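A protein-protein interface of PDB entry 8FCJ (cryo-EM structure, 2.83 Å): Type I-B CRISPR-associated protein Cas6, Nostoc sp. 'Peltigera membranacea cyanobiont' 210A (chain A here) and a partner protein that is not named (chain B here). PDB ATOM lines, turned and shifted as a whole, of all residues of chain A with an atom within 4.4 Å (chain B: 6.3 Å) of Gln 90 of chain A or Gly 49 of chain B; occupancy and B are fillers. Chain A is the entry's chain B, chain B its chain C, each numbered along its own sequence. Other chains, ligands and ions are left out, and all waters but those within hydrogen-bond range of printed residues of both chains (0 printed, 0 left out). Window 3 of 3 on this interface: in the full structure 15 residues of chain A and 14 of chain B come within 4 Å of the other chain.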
ATOM      1  N   PRO A  85     -22.913   6.385 -31.040  1.00  0.00           N
ATOM      2  CA  PRO A  85     -22.107   7.602 -31.241  1.00  0.00           C
ATOM      3  C   PRO A  85     -22.917   8.804 -31.683  1.00  0.00           C
ATOM      4  O   PRO A  85     -22.500   9.940 -31.425  1.00  0.00           O
ATOM      5  CB  PRO A  85     -21.093   7.184 -32.314  1.00  0.00           C
ATOM      6  CG  PRO A  85     -21.711   6.025 -32.996  1.00  0.00           C
ATOM      7  CD  PRO A  85     -22.488   5.303 -31.948  1.00  0.00           C
ATOM      8  N   TYR A  86     -24.056   8.599 -32.339  1.00  0.00           N
ATOM      9  CA  TYR A  86     -24.884   9.706 -32.797  1.00  0.00           C
ATOM     10  C   TYR A  86     -25.753  10.296 -31.695  1.00  0.00           C
ATOM     11  O   TYR A  86     -26.137  11.466 -31.791  1.00  0.00           O
ATOM     12  CB  TYR A  86     -25.792   9.271 -33.957  1.00  0.00           C
ATOM     13  CG  TYR A  86     -25.086   8.707 -35.177  1.00  0.00           C
ATOM     14  CD1 TYR A  86     -24.277   7.581 -35.093  1.00  0.00           C
ATOM     15  CD2 TYR A  86     -25.238   9.307 -36.420  1.00  0.00           C
ATOM     16  CE1 TYR A  86     -23.641   7.072 -36.205  1.00  0.00           C
ATOM     17  CE2 TYR A  86     -24.604   8.804 -37.539  1.00  0.00           C
ATOM     18  CZ  TYR A  86     -23.807   7.687 -37.425  1.00  0.00           C
ATOM     19  OH  TYR A  86     -23.173   7.181 -38.537  1.00  0.00           O
ATOM     20  N   LEU A  87     -26.067   9.523 -30.660  1.00  0.00           N
ATOM     21  CA  LEU A  87     -27.004   9.939 -29.621  1.00  0.00           C
ATOM     22  C   LEU A  87     -26.346  10.242 -28.286  1.00  0.00           C
ATOM     23  O   LEU A  87     -26.717  11.219 -27.633  1.00  0.00           O
ATOM     24  CB  LEU A  87     -28.069   8.858 -29.414  1.00  0.00           C
ATOM     25  CG  LEU A  87     -29.417   9.057 -30.109  1.00  0.00           C
ATOM     26  CD1 LEU A  87     -29.224   9.428 -31.564  1.00  0.00           C
ATOM     27  CD2 LEU A  87     -30.259   7.800 -29.990  1.00  0.00           C
ATOM     28  N   ALA A  88     -25.384   9.429 -27.859  1.00  0.00           N
ATOM     29  CA  ALA A  88     -24.776   9.587 -26.541  1.00  0.00           C
ATOM     30  C   ALA A  88     -23.979  10.883 -26.493  1.00  0.00           C
ATOM     31  O   ALA A  88     -22.969  11.027 -27.188  1.00  0.00           O
ATOM     32  CB  ALA A  88     -23.886   8.390 -26.226  1.00  0.00           C
ATOM     33  N   GLY A  89     -24.428  11.827 -25.669  1.00  0.00           N
ATOM     34  CA  GLY A  89     -23.746  13.090 -25.503  1.00  0.00           C
ATOM     35  C   GLY A  89     -24.136  14.170 -26.487  1.00  0.00           C
ATOM     36  O   GLY A  89     -23.658  15.304 -26.355  1.00  0.00           O
ATOM     37  N   GLN A  90     -24.986  13.865 -27.462  1.00  0.00           N
ATOM     38  CA  GLN A  90     -25.384  14.844 -28.458  1.00  0.00           C
ATOM     39  C   GLN A  90     -26.694  15.512 -28.049  1.00  0.00           C
ATOM     40  O   GLN A  90     -27.293  15.194 -27.019  1.00  0.00           O
ATOM     41  CB  GLN A  90     -25.498  14.182 -29.830  1.00  0.00           C
ATOM     42  CG  GLN A  90     -24.288  14.406 -30.721  1.00  0.00           C
ATOM     43  CD  GLN A  90     -23.008  13.854 -30.124  1.00  0.00           C
ATOM     44  OE1 GLN A  90     -23.033  12.922 -29.319  1.00  0.00           O
ATOM     45  NE2 GLN A  90     -21.878  14.428 -30.516  1.00  0.00           N
ATOM     46  N   ALA A  91     -27.149  16.455 -28.871  1.00  0.00           N
ATOM     47  CA  ALA A  91     -28.351  17.224 -28.589  1.00  0.00           C
ATOM     48  C   ALA A  91     -29.264  17.229 -29.805  1.00  0.00           C
ATOM     49  O   ALA A  91     -28.795  17.289 -30.946  1.00  0.00           O
ATOM     50  CB  ALA A  91     -28.008  18.661 -28.188  1.00  0.00           C
ATOM     51  N   GLN A 100     -30.853  17.929 -24.495  1.00  0.00           N
ATOM     52  CA  GLN A 100     -29.541  17.320 -24.344  1.00  0.00           C
ATOM     53  C   GLN A 100     -29.665  15.902 -23.803  1.00  0.00           C
ATOM     54  O   GLN A 100     -30.466  15.638 -22.901  1.00  0.00           O
ATOM     55  CB  GLN A 100     -28.658  18.156 -23.413  1.00  0.00           C
ATOM     56  CG  GLN A 100     -27.257  17.602 -23.221  1.00  0.00           C
ATOM     57  CD  GLN A 100     -26.268  18.159 -24.221  1.00  0.00           C
ATOM     58  OE1 GLN A 100     -26.555  19.129 -24.921  1.00  0.00           O
ATOM     59  NE2 GLN A 100     -25.093  17.546 -24.296  1.00  0.00           N
ATOM     60  N   LEU A 101     -28.871  14.996 -24.365  1.00  0.00           N
ATOM     61  CA  LEU A 101     -28.779  13.618 -23.905  1.00  0.00           C
ATOM     62  C   LEU A 101     -27.381  13.358 -23.364  1.00  0.00           C
ATOM     63  O   LEU A 101     -26.389  13.797 -23.951  1.00  0.00           O
ATOM     64  CB  LEU A 101     -29.086  12.636 -25.038  1.00  0.00           C
ATOM     65  CG  LEU A 101     -30.351  12.884 -25.858  1.00  0.00           C
ATOM     66  CD1 LEU A 101     -30.270  12.160 -27.189  1.00  0.00           C
ATOM     67  CD2 LEU A 101     -31.579  12.442 -25.087  1.00  0.00           C
ATOM     68  N   TYR B  45     -16.042  12.996 -21.888  1.00  0.00           N
ATOM     69  CA  TYR B  45     -15.940  13.793 -23.100  1.00  0.00           C
ATOM     70  C   TYR B  45     -14.485  14.004 -23.493  1.00  0.00           C
ATOM     71  O   TYR B  45     -13.589  14.059 -22.648  1.00  0.00           O
ATOM     72  CB  TYR B  45     -16.626  15.145 -22.918  1.00  0.00           C
ATOM     73  CG  TYR B  45     -18.130  15.083 -23.008  1.00  0.00           C
ATOM     74  CD1 TYR B  45     -18.764  14.933 -24.232  1.00  0.00           C
ATOM     75  CD2 TYR B  45     -18.917  15.183 -21.871  1.00  0.00           C
ATOM     76  CE1 TYR B  45     -20.138  14.878 -24.321  1.00  0.00           C
ATOM     77  CE2 TYR B  45     -20.292  15.130 -21.950  1.00  0.00           C
ATOM     78  CZ  TYR B  45     -20.897  14.978 -23.177  1.00  0.00           C
ATOM     79  OH  TYR B  45     -22.268  14.926 -23.258  1.00  0.00           O
ATOM     80  N   TRP B  46     -14.262  14.122 -24.796  1.00  0.00           N
ATOM     81  CA  TRP B  46     -12.945  14.389 -25.361  1.00  0.00           C
ATOM     82  C   TRP B  46     -13.153  15.373 -26.507  1.00  0.00           C
ATOM     83  O   TRP B  46     -14.200  16.021 -26.606  1.00  0.00           O
ATOM     84  CB  TRP B  46     -12.261  13.078 -25.780  1.00  0.00           C
ATOM     85  CG  TRP B  46     -10.759  13.146 -25.860  1.00  0.00           C
ATOM     86  CD1 TRP B  46      -9.981  12.693 -26.883  1.00  0.00           C
ATOM     87  CD2 TRP B  46      -9.856  13.673 -24.877  1.00  0.00           C
ATOM     88  NE1 TRP B  46      -8.656  12.914 -26.606  1.00  0.00           N
ATOM     89  CE2 TRP B  46      -8.553  13.515 -25.381  1.00  0.00           C
ATOM     90  CE3 TRP B  46     -10.026  14.268 -23.624  1.00  0.00           C
ATOM     91  CZ2 TRP B  46      -7.427  13.930 -24.678  1.00  0.00           C
ATOM     92  CZ3 TRP B  46      -8.906  14.679 -22.930  1.00  0.00           C
ATOM     93  CH2 TRP B  46      -7.624  14.507 -23.457  1.00  0.00           C
ATOM     94  N   ASN B  47     -12.155  15.511 -27.376  1.00  0.00           N
ATOM     95  CA  ASN B  47     -12.285  16.434 -28.497  1.00  0.00           C
ATOM     96  C   ASN B  47     -13.458  16.037 -29.384  1.00  0.00           C
ATOM     97  O   ASN B  47     -13.892  14.883 -29.400  1.00  0.00           O
ATOM     98  CB  ASN B  47     -11.000  16.472 -29.320  1.00  0.00           C
ATOM     99  CG  ASN B  47     -10.288  15.142 -29.353  1.00  0.00           C
ATOM    100  OD1 ASN B  47     -10.788  14.172 -29.917  1.00  0.00           O
ATOM    101  ND2 ASN B  47      -9.107  15.091 -28.752  1.00  0.00           N
ATOM    102  N   ASN B  48     -13.979  17.019 -30.119  1.00  0.00           N
ATOM    103  CA  ASN B  48     -15.178  16.903 -30.944  1.00  0.00           C
ATOM    104  C   ASN B  48     -16.436  16.648 -30.123  1.00  0.00           C
ATOM    105  O   ASN B  48     -17.494  16.366 -30.696  1.00  0.00           O
ATOM    106  CB  ASN B  48     -15.035  15.817 -32.020  1.00  0.00           C
ATOM    107  CG  ASN B  48     -13.712  15.887 -32.750  1.00  0.00           C
ATOM    108  OD1 ASN B  48     -12.685  15.441 -32.242  1.00  0.00           O
ATOM    109  ND2 ASN B  48     -13.730  16.447 -33.953  1.00  0.00           N
ATOM    110  N   GLY B  49     -16.352  16.745 -28.802  1.00  0.00           N
ATOM    111  CA  GLY B  49     -17.522  16.555 -27.959  1.00  0.00           C
ATOM    112  C   GLY B  49     -18.117  15.167 -28.032  1.00  0.00           C
ATOM    113  O   GLY B  49     -19.339  15.011 -27.922  1.00  0.00           O
ATOM    114  N   LYS B  50     -17.280  14.152 -28.210  1.00  0.00           N
ATOM    115  CA  LYS B  50     -17.726  12.771 -28.283  1.00  0.00           C
ATOM    116  C   LYS B  50     -17.211  11.997 -27.078  1.00  0.00           C
ATOM    117  O   LYS B  50     -16.256  12.410 -26.415  1.00  0.00           O
ATOM    118  CB  LYS B  50     -17.255  12.106 -29.578  1.00  0.00           C
ATOM    119  CG  LYS B  50     -17.572  12.912 -30.821  1.00  0.00           C
ATOM    120  CD  LYS B  50     -17.486  12.059 -32.071  1.00  0.00           C
ATOM    121  CE  LYS B  50     -18.631  12.367 -33.019  1.00  0.00           C
ATOM    122  NZ  LYS B  50     -19.919  12.520 -32.292  1.00  0.00           N
ATOM    123  N   ILE B  51     -17.857  10.872 -26.800  1.00  0.00           N
ATOM    124  CA  ILE B  51     -17.566  10.104 -25.595  1.00  0.00           C
ATOM    125  C   ILE B  51     -16.401   9.165 -25.861  1.00  0.00           C
ATOM    126  O   ILE B  51     -16.441   8.348 -26.788  1.00  0.00           O
ATOM    127  CB  ILE B  51     -18.810   9.332 -25.136  1.00  0.00           C
ATOM    128  CG1 ILE B  51     -20.025  10.260 -25.135  1.00  0.00           C
ATOM    129  CG2 ILE B  51     -18.584   8.718 -23.767  1.00  0.00           C
ATOM    130  CD1 ILE B  51     -20.211  11.028 -23.851  1.00  0.00           C
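Printed residues of chain B that touch a printed residue of chain A: Tyr 45, Gly 49, Lys 50 and Ile 51.
Hydrophobic or aromatic side chains of chain B that line the printed part of chain A: Tyr 45 and Ile 51.
Of the 9 printed residues of chain A, 5 touch a printed residue of chain B.
Among the printed residues, 6 pairs touch across the chains.
Among the printed residues, no Asp or Glu carboxylate lies within 4 Å of a Lys or Arg side-chain nitrogen of the other chain.
NZ of Lys 50 of chain B sits close to NE2 of Gln 90 of chain A (3.3 Å).
The backbone carbonyl oxygen (O) of Gly 89 of chain A sits close to the side-chain hydroxyl (OH) of Tyr 45 of chain B, 3.4 Å away.
O of Pro 85 of chain A touches NZ of Lys 50 of chain B, at 3.8 Å.
Ala 88 of chain A touches Ile 51 of chain B.
O of Gly 49 of chain B touches NE2 of Gln 90 of chain A (3.7 Å).
NE2 of Gln 100 of chain A touches OH of Tyr 45 of chain B, at 3.99 Å.
The backbone carbonyl oxygen of Gly 89 of chain A lies within hydrogen-bond range of the side-chain amide nitrogen of Gln 100 of chain A.
The backbone NH (N) of Leu 101 of chain A sits at hydrogen-bond distance from the backbone carbonyl oxygen (O) of Gln 90 of chain A.
O of Ala 88 of chain A sits close to OE1 of Gln 90 of chain A (2.9 Å).
N of Gly 89 of chain A sits close to O of Leu 101 of chain A (3.3 Å).
Printed residues of chain B within 4 Å of Ala 88 of chain A: Ile 51 (3.7 Å).
Printed residues of chain B within 4 Å of Gly 89 of chain A: Tyr 45.
Of chain B, only Gly 49 and Lys 50 come within 4 Å of Gln 90 of chain A.
Leu 101 of chain A touches none of the printed residues of chain B.
Gly 49 of chain B touches one residue of chain A.
Printed residues of chain A within 4 Å of Lys 50 of chain B: Pro 85 (3.8 Å) and Gln 90 (3.3 Å).
The nearest residue of chain B that does not touch Gln 90 of chain A is Asn 48 of chain B (4.8 Å).
The nearest printed residue of chain A that does not touch Gly 49 of chain B is Gly 89 of chain A (4.6 Å).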
